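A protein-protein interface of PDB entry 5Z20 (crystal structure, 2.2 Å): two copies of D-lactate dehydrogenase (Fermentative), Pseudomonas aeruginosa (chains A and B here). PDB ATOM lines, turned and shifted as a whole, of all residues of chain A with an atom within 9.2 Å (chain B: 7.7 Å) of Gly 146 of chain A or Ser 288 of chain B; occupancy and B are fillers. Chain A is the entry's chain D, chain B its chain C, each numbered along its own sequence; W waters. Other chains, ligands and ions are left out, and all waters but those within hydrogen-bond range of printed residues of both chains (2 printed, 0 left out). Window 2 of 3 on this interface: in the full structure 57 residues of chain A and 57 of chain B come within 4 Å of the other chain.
The backbone carbonyl oxygen (O) of Glu 285 of chain B is in hydrogen-bond range of the backbone NH (N) of Phe 148 of chain A, at 3.1 Å.
The backbone carbonyl oxygen of Gly 146 of chain A sits at hydrogen-bond distance from the backbone NH of Arg 287 of chain B (3.0 Å).
N of Ser 288 of chain B is in hydrogen-bond range of O of Gly 146 of chain A (3.3 Å).
The backbone carbonyl oxygen (O) of Leu 301 of chain B is in hydrogen-bond range of the guanidinium group (NH1) of Arg 144 of chain A, at 2.8 Å.
The side-chain carboxylate (OE2) of Glu 285 of chain B is in salt-bridge range of the guanidinium group (NH2) of Arg 287 of chain B (2.4 Å).
The backbone carbonyl oxygen (O) of Ala 139 of chain A sits at hydrogen-bond distance from the side-chain hydroxyl (OG1) of Thr 143 of chain A.
The guanidinium group of Arg 144 of chain A sits at hydrogen-bond distance from the side-chain hydroxyl of Tyr 140 of chain A, 3.0 Å away.
The backbone carbonyl oxygen of Arg 142 of chain A lies within hydrogen-bond range of the backbone NH of Asp 147 of chain A (2.8 Å).
The backbone carbonyl oxygen (O) of Ser 149 of chain A sits at hydrogen-bond distance from the guanidinium group (NH1) of Arg 142 of chain A, 2.9 Å away.
OG of Ser 149 of chain A lies within hydrogen-bond range of OD1 of Asp 147 of chain A.
Among the printed residues, pairs that only touch across the chains: Thr 143 of chain A with Leu 301 of chain B (3.3 Å), Glu 145 of chain A with Ser 288 of chain B (3.3 Å), Asp 147 of chain A with Asp 286 of chain B (3.5 Å), Phe 148 of chain A with Ile 282 of chain B (3.2 Å), Phe 148 of chain A with Leu 297 of chain B (3.97 Å) and Ser 149 of chain A with Glu 285 of chain B (3.6 Å).
Ala 139 of chain A touches none of the printed residues of chain B.
Arg 142 of chain A touches none of the printed residues of chain B.
Of the printed residues of chain B, Arg 144 of chain A touches Leu 301.
Gly 146 of chain A touches just these residues of chain B: Arg 287 (3.0 Å) and Ser 288 (3.3 Å).
Printed residues of chain A within 4 Å of Arg 287 of chain B: Gly 146.
Of chain A, only Glu 145 and Gly 146 come within 4 Å of Ser 288 of chain B.
No residue of chain A comes within 4 Å of Asp 289 of chain B.
The nearest residue of chain B that does not touch Gly 146 of chain A is Asp 286 of chain B (4.1 Å).
The nearest residue of chain A that does not touch Ser 288 of chain B is Asp 147 of chain A (4.1 Å).
Hydrophobic or aromatic side chains of chain A within 4 Å of the printed part of chain B: Phe 148.
Of the 11 printed residues of chain B, 7 touch a printed residue of chain A.
Printed residues of chain B that touch a printed residue of chain A: Ile 282, Glu 285, Asp 286, Arg 287, Ser 288, Leu 297 and Leu 301.
Hydrophobic or aromatic side chains of chain B within 4 Å of the printed part of chain A: Ile 282, Leu 297 and Leu 301.
Among the printed residues, 10 pairs touch across the chains.
Among the printed residues, no Asp or Glu carboxylate lies within 4 Å of a Lys or Arg side-chain nitrogen of the other chain.
No position is printed for both chains.
Of the 10 pairs that touch across the chains among the printed residues, none has its exchanged pair printed and touching as well.
Water W1 lies within hydrogen-bond range of the side-chain carboxylate of Asp 286 of chain B, the side-chain carboxylate of Asp 147 of chain A and the side-chain hydroxyl of Ser 288 of chain B.
Water W2 bridges the backbone carbonyl oxygen of Ser 288 of chain B and the backbone carbonyl oxygen of Glu 145 of chain A.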
ATOM      1  N   ALA A 139     -19.517 -35.971 -33.824  1.00  0.00           N
ATOM      2  CA  ALA A 139     -19.982 -35.296 -32.626  1.00  0.00           C
ATOM      3  C   ALA A 139     -19.086 -35.528 -31.462  1.00  0.00           C
ATOM      4  O   ALA A 139     -18.744 -34.594 -30.729  1.00  0.00           O
ATOM      5  CB  ALA A 139     -21.450 -35.691 -32.284  1.00  0.00           C
ATOM      6  N   TYR A 140     -18.756 -36.805 -31.227  1.00  0.00           N
ATOM      7  CA  TYR A 140     -17.874 -37.169 -30.116  1.00  0.00           C
ATOM      8  C   TYR A 140     -16.576 -36.388 -30.108  1.00  0.00           C
ATOM      9  O   TYR A 140     -16.196 -35.777 -29.132  1.00  0.00           O
ATOM     10  CB  TYR A 140     -17.566 -38.637 -30.164  1.00  0.00           C
ATOM     11  CG  TYR A 140     -16.536 -39.047 -29.113  1.00  0.00           C
ATOM     12  CD1 TYR A 140     -16.905 -39.136 -27.766  1.00  0.00           C
ATOM     13  CD2 TYR A 140     -15.243 -39.352 -29.471  1.00  0.00           C
ATOM     14  CE1 TYR A 140     -15.994 -39.463 -26.794  1.00  0.00           C
ATOM     15  CE2 TYR A 140     -14.291 -39.752 -28.509  1.00  0.00           C
ATOM     16  CZ  TYR A 140     -14.667 -39.825 -27.185  1.00  0.00           C
ATOM     17  OH  TYR A 140     -13.790 -40.267 -26.248  1.00  0.00           O
ATOM     18  N   ASN A 141     -15.892 -36.368 -31.231  1.00  0.00           N
ATOM     19  CA  ASN A 141     -14.684 -35.591 -31.368  1.00  0.00           C
ATOM     20  C   ASN A 141     -14.896 -34.084 -31.192  1.00  0.00           C
ATOM     21  O   ASN A 141     -14.087 -33.424 -30.648  1.00  0.00           O
ATOM     22  CB  ASN A 141     -13.954 -35.919 -32.664  1.00  0.00           C
ATOM     23  CG  ASN A 141     -13.364 -37.306 -32.661  1.00  0.00           C
ATOM     24  OD1 ASN A 141     -13.043 -37.820 -31.628  1.00  0.00           O
ATOM     25  ND2 ASN A 141     -13.250 -37.884 -33.794  1.00  0.00           N
ATOM     26  N   ARG A 142     -16.022 -33.570 -31.618  1.00  0.00           N
ATOM     27  CA  ARG A 142     -16.295 -32.158 -31.364  1.00  0.00           C
ATOM     28  C   ARG A 142     -16.489 -31.799 -29.871  1.00  0.00           C
ATOM     29  O   ARG A 142     -15.818 -30.907 -29.334  1.00  0.00           O
ATOM     30  CB  ARG A 142     -17.526 -31.676 -32.126  1.00  0.00           C
ATOM     31  CG  ARG A 142     -17.325 -31.602 -33.630  1.00  0.00           C
ATOM     32  CD  ARG A 142     -18.528 -30.889 -34.248  1.00  0.00           C
ATOM     33  NE  ARG A 142     -18.487 -31.005 -35.713  1.00  0.00           N
ATOM     34  CZ  ARG A 142     -19.422 -30.546 -36.552  1.00  0.00           C
ATOM     35  NH1 ARG A 142     -20.525 -29.941 -36.096  1.00  0.00           N
ATOM     36  NH2 ARG A 142     -19.264 -30.734 -37.831  1.00  0.00           N
ATOM     37  N   THR A 143     -17.365 -32.541 -29.202  1.00  0.00           N
ATOM     38  CA  THR A 143     -17.702 -32.164 -27.838  1.00  0.00           C
ATOM     39  C   THR A 143     -16.538 -32.371 -26.948  1.00  0.00           C
ATOM     40  O   THR A 143     -16.303 -31.633 -25.987  1.00  0.00           O
ATOM     41  CB  THR A 143     -18.922 -32.892 -27.308  1.00  0.00           C
ATOM     42  OG1 THR A 143     -18.697 -34.304 -27.261  1.00  0.00           O
ATOM     43  CG2 THR A 143     -20.133 -32.603 -28.216  1.00  0.00           C
ATOM     44  N   ARG A 144     -15.770 -33.384 -27.255  1.00  0.00           N
ATOM     45  CA  ARG A 144     -14.558 -33.623 -26.550  1.00  0.00           C
ATOM     46  C   ARG A 144     -13.555 -32.481 -26.498  1.00  0.00           C
ATOM     47  O   ARG A 144     -12.820 -32.380 -25.600  1.00  0.00           O
ATOM     48  CB  ARG A 144     -13.896 -34.863 -27.042  1.00  0.00           C
ATOM     49  CG  ARG A 144     -13.484 -35.622 -25.854  1.00  0.00           C
ATOM     50  CD  ARG A 144     -13.722 -37.094 -25.961  1.00  0.00           C
ATOM     51  NE  ARG A 144     -12.401 -37.645 -25.866  1.00  0.00           N
ATOM     52  CZ  ARG A 144     -11.929 -38.346 -24.855  1.00  0.00           C
ATOM     53  NH1 ARG A 144     -12.702 -38.661 -23.847  1.00  0.00           N
ATOM     54  NH2 ARG A 144     -10.690 -38.766 -24.899  1.00  0.00           N
ATOM     55  N   GLU A 145     -13.572 -31.619 -27.475  1.00  0.00           N
ATOM     56  CA  GLU A 145     -12.695 -30.439 -27.477  1.00  0.00           C
ATOM     57  C   GLU A 145     -13.483 -29.188 -27.264  1.00  0.00           C
ATOM     58  O   GLU A 145     -12.989 -28.100 -27.430  1.00  0.00           O
ATOM     59  CB  GLU A 145     -11.850 -30.379 -28.765  1.00  0.00           C
ATOM     60  CG  GLU A 145     -12.679 -30.311 -30.049  1.00  0.00           C
ATOM     61  CD  GLU A 145     -11.881 -30.119 -31.341  1.00  0.00           C
ATOM     62  OE1 GLU A 145     -10.783 -29.549 -31.313  1.00  0.00           O
ATOM     63  OE2 GLU A 145     -12.401 -30.472 -32.397  1.00  0.00           O
ATOM     64  N   GLY A 146     -14.719 -29.309 -26.807  1.00  0.00           N
ATOM     65  CA  GLY A 146     -15.491 -28.130 -26.486  1.00  0.00           C
ATOM     66  C   GLY A 146     -16.154 -27.451 -27.693  1.00  0.00           C
ATOM     67  O   GLY A 146     -16.605 -26.314 -27.582  1.00  0.00           O
ATOM     68  N   ASP A 147     -16.241 -28.161 -28.801  1.00  0.00           N
ATOM     69  CA  ASP A 147     -17.015 -27.716 -29.910  1.00  0.00           C
ATOM     70  C   ASP A 147     -18.433 -28.294 -29.838  1.00  0.00           C
ATOM     71  O   ASP A 147     -18.635 -29.473 -30.121  1.00  0.00           O
ATOM     72  CB  ASP A 147     -16.326 -28.146 -31.251  1.00  0.00           C
ATOM     73  CG  ASP A 147     -17.130 -27.737 -32.471  1.00  0.00           C
ATOM     74  OD1 ASP A 147     -18.187 -27.049 -32.320  1.00  0.00           O
ATOM     75  OD2 ASP A 147     -16.639 -28.002 -33.596  1.00  0.00           O
ATOM     76  N   PHE A 148     -19.397 -27.472 -29.461  1.00  0.00           N
ATOM     77  CA  PHE A 148     -20.763 -27.933 -29.308  1.00  0.00           C
ATOM     78  C   PHE A 148     -21.615 -27.452 -30.492  1.00  0.00           C
ATOM     79  O   PHE A 148     -22.814 -27.389 -30.354  1.00  0.00           O
ATOM     80  CB  PHE A 148     -21.315 -27.435 -27.987  1.00  0.00           C
ATOM     81  CG  PHE A 148     -20.446 -27.793 -26.837  1.00  0.00           C
ATOM     82  CD1 PHE A 148     -20.369 -29.106 -26.379  1.00  0.00           C
ATOM     83  CD2 PHE A 148     -19.696 -26.830 -26.181  1.00  0.00           C
ATOM     84  CE1 PHE A 148     -19.595 -29.442 -25.263  1.00  0.00           C
ATOM     85  CE2 PHE A 148     -18.879 -27.182 -25.108  1.00  0.00           C
ATOM     86  CZ  PHE A 148     -18.833 -28.491 -24.635  1.00  0.00           C
ATOM     87  N   SER A 149     -20.991 -27.121 -31.635  1.00  0.00           N
ATOM     88  CA  SER A 149     -21.740 -26.716 -32.818  1.00  0.00           C
ATOM     89  C   SER A 149     -22.242 -27.952 -33.564  1.00  0.00           C
ATOM     90  O   SER A 149     -21.625 -29.032 -33.541  1.00  0.00           O
ATOM     91  CB  SER A 149     -20.926 -25.815 -33.732  1.00  0.00           C
ATOM     92  OG  SER A 149     -19.812 -26.498 -34.324  1.00  0.00           O
ATOM     93  N   ILE B 282     -23.428 -22.908 -23.135  1.00  0.00           N
ATOM     94  CA  ILE B 282     -22.285 -23.720 -23.657  1.00  0.00           C
ATOM     95  C   ILE B 282     -22.717 -24.328 -25.019  1.00  0.00           C
ATOM     96  O   ILE B 282     -22.131 -24.108 -26.045  1.00  0.00           O
ATOM     97  CB  ILE B 282     -22.004 -24.840 -22.602  1.00  0.00           C
ATOM     98  CG1 ILE B 282     -21.472 -24.259 -21.306  1.00  0.00           C
ATOM     99  CG2 ILE B 282     -20.984 -25.830 -23.079  1.00  0.00           C
ATOM    100  CD1 ILE B 282     -21.298 -25.248 -20.138  1.00  0.00           C
ATOM    101  N   GLU B 285     -22.744 -23.771 -29.632  1.00  0.00           N
ATOM    102  CA  GLU B 285     -21.710 -22.957 -30.186  1.00  0.00           C
ATOM    103  C   GLU B 285     -20.351 -23.647 -30.123  1.00  0.00           C
ATOM    104  O   GLU B 285     -20.141 -24.504 -29.328  1.00  0.00           O
ATOM    105  CB  GLU B 285     -21.745 -21.560 -29.560  1.00  0.00           C
ATOM    106  CG  GLU B 285     -21.519 -21.554 -28.085  1.00  0.00           C
ATOM    107  CD  GLU B 285     -22.344 -20.523 -27.324  1.00  0.00           C
ATOM    108  OE1 GLU B 285     -23.395 -20.904 -26.727  1.00  0.00           O
ATOM    109  OE2 GLU B 285     -21.923 -19.354 -27.325  1.00  0.00           O
ATOM    110  N   ASP B 286     -19.451 -23.277 -31.009  1.00  0.00           N
ATOM    111  CA  ASP B 286     -18.108 -23.816 -30.983  1.00  0.00           C
ATOM    112  C   ASP B 286     -17.320 -23.055 -29.972  1.00  0.00           C
ATOM    113  O   ASP B 286     -16.919 -21.959 -30.233  1.00  0.00           O
ATOM    114  CB  ASP B 286     -17.429 -23.651 -32.346  1.00  0.00           C
ATOM    115  CG  ASP B 286     -16.023 -24.233 -32.364  1.00  0.00           C
ATOM    116  OD1 ASP B 286     -15.523 -24.758 -31.337  1.00  0.00           O
ATOM    117  OD2 ASP B 286     -15.430 -24.153 -33.414  1.00  0.00           O
ATOM    118  N   ARG B 287     -17.010 -23.651 -28.842  1.00  0.00           N
ATOM    119  CA  ARG B 287     -16.217 -22.975 -27.799  1.00  0.00           C
ATOM    120  C   ARG B 287     -14.859 -23.584 -27.678  1.00  0.00           C
ATOM    121  O   ARG B 287     -14.211 -23.548 -26.620  1.00  0.00           O
ATOM    122  CB  ARG B 287     -16.937 -23.113 -26.461  1.00  0.00           C
ATOM    123  CG  ARG B 287     -18.297 -22.504 -26.574  1.00  0.00           C
ATOM    124  CD  ARG B 287     -18.993 -22.373 -25.249  1.00  0.00           C
ATOM    125  NE  ARG B 287     -19.938 -21.281 -25.389  1.00  0.00           N
ATOM    126  CZ  ARG B 287     -19.709 -20.016 -25.057  1.00  0.00           C
ATOM    127  NH1 ARG B 287     -18.591 -19.665 -24.458  1.00  0.00           N
ATOM    128  NH2 ARG B 287     -20.649 -19.109 -25.293  1.00  0.00           N
ATOM    129  N   SER B 288     -14.406 -24.190 -28.749  1.00  0.00           N
ATOM    130  CA  SER B 288     -13.171 -24.983 -28.636  1.00  0.00           C
ATOM    131  C   SER B 288     -11.948 -24.083 -28.443  1.00  0.00           C
ATOM    132  O   SER B 288     -10.903 -24.584 -28.135  1.00  0.00           O
ATOM    133  CB  SER B 288     -12.964 -25.866 -29.875  1.00  0.00           C
ATOM    134  OG  SER B 288     -12.906 -25.116 -31.066  1.00  0.00           O
ATOM    135  N   ASP B 289     -12.047 -22.802 -28.784  1.00  0.00           N
ATOM    136  CA  ASP B 289     -10.890 -21.902 -28.724  1.00  0.00           C
ATOM    137  C   ASP B 289     -10.588 -21.429 -27.285  1.00  0.00           C
ATOM    138  O   ASP B 289      -9.580 -20.887 -27.081  1.00  0.00           O
ATOM    139  CB  ASP B 289     -11.060 -20.683 -29.680  1.00  0.00           C
ATOM    140  CG  ASP B 289     -11.090 -21.102 -31.164  1.00  0.00           C
ATOM    141  OD1 ASP B 289     -10.470 -22.138 -31.553  1.00  0.00           O
ATOM    142  OD2 ASP B 289     -11.718 -20.381 -31.982  1.00  0.00           O
ATOM    143  N   GLN B 290     -11.489 -21.600 -26.328  1.00  0.00           N
ATOM    144  CA  GLN B 290     -11.273 -21.166 -24.964  1.00  0.00           C
ATOM    145  C   GLN B 290     -11.354 -22.294 -23.991  1.00  0.00           C
ATOM    146  O   GLN B 290     -11.981 -23.253 -24.244  1.00  0.00           O
ATOM    147  CB  GLN B 290     -12.313 -20.151 -24.529  1.00  0.00           C
ATOM    148  CG  GLN B 290     -12.608 -19.042 -25.497  1.00  0.00           C
ATOM    149  CD  GLN B 290     -11.426 -18.161 -25.742  1.00  0.00           C
ATOM    150  OE1 GLN B 290     -10.630 -17.893 -24.851  1.00  0.00           O
ATOM    151  NE2 GLN B 290     -11.311 -17.688 -26.963  1.00  0.00           N
ATOM    152  N   PRO B 291     -10.732 -22.137 -22.846  1.00  0.00           N
ATOM    153  CA  PRO B 291     -10.937 -23.109 -21.800  1.00  0.00           C
ATOM    154  C   PRO B 291     -12.403 -23.292 -21.467  1.00  0.00           C
ATOM    155  O   PRO B 291     -13.172 -22.332 -21.427  1.00  0.00           O
ATOM    156  CB  PRO B 291     -10.245 -22.457 -20.608  1.00  0.00           C
ATOM    157  CG  PRO B 291      -9.167 -21.595 -21.199  1.00  0.00           C
ATOM    158  CD  PRO B 291      -9.805 -21.055 -22.452  1.00  0.00           C
ATOM    159  N   LEU B 292     -12.792 -24.510 -21.208  1.00  0.00           N
ATOM    160  CA  LEU B 292     -14.104 -24.800 -20.702  1.00  0.00           C
ATOM    161  C   LEU B 292     -14.173 -24.545 -19.217  1.00  0.00           C
ATOM    162  O   LEU B 292     -13.355 -25.062 -18.489  1.00  0.00           O
ATOM    163  CB  LEU B 292     -14.376 -26.292 -21.035  1.00  0.00           C
ATOM    164  CG  LEU B 292     -15.796 -26.750 -20.768  1.00  0.00           C
ATOM    165  CD1 LEU B 292     -16.711 -26.033 -21.712  1.00  0.00           C
ATOM    166  CD2 LEU B 292     -15.867 -28.270 -20.982  1.00  0.00           C
ATOM    167  N   LEU B 297     -18.505 -30.848 -16.492  1.00  0.00           N
ATOM    168  CA  LEU B 297     -18.611 -31.269 -17.912  1.00  0.00           C
ATOM    169  C   LEU B 297     -17.261 -31.663 -18.440  1.00  0.00           C
ATOM    170  O   LEU B 297     -17.116 -32.676 -19.089  1.00  0.00           O
ATOM    171  CB  LEU B 297     -19.183 -30.175 -18.762  1.00  0.00           C
ATOM    172  CG  LEU B 297     -19.417 -30.576 -20.225  1.00  0.00           C
ATOM    173  CD1 LEU B 297     -20.305 -31.734 -20.418  1.00  0.00           C
ATOM    174  CD2 LEU B 297     -19.995 -29.378 -20.949  1.00  0.00           C
ATOM    175  N   LEU B 301     -16.371 -35.341 -20.064  1.00  0.00           N
ATOM    176  CA  LEU B 301     -15.765 -35.474 -21.357  1.00  0.00           C
ATOM    177  C   LEU B 301     -14.454 -36.261 -21.390  1.00  0.00           C
ATOM    178  O   LEU B 301     -14.124 -36.750 -22.392  1.00  0.00           O
ATOM    179  CB  LEU B 301     -15.553 -34.106 -22.001  1.00  0.00           C
ATOM    180  CG  LEU B 301     -16.841 -33.335 -22.315  1.00  0.00           C
ATOM    181  CD1 LEU B 301     -16.513 -31.907 -22.656  1.00  0.00           C
ATOM    182  CD2 LEU B 301     -17.649 -34.011 -23.440  1.00  0.00           C
HETATM  183  O   HOH W   1     -13.898 -26.188 -34.203  1.00  0.00           O
HETATM  184  O   HOH W   2     -10.396 -27.201 -27.736  1.00  0.00           O
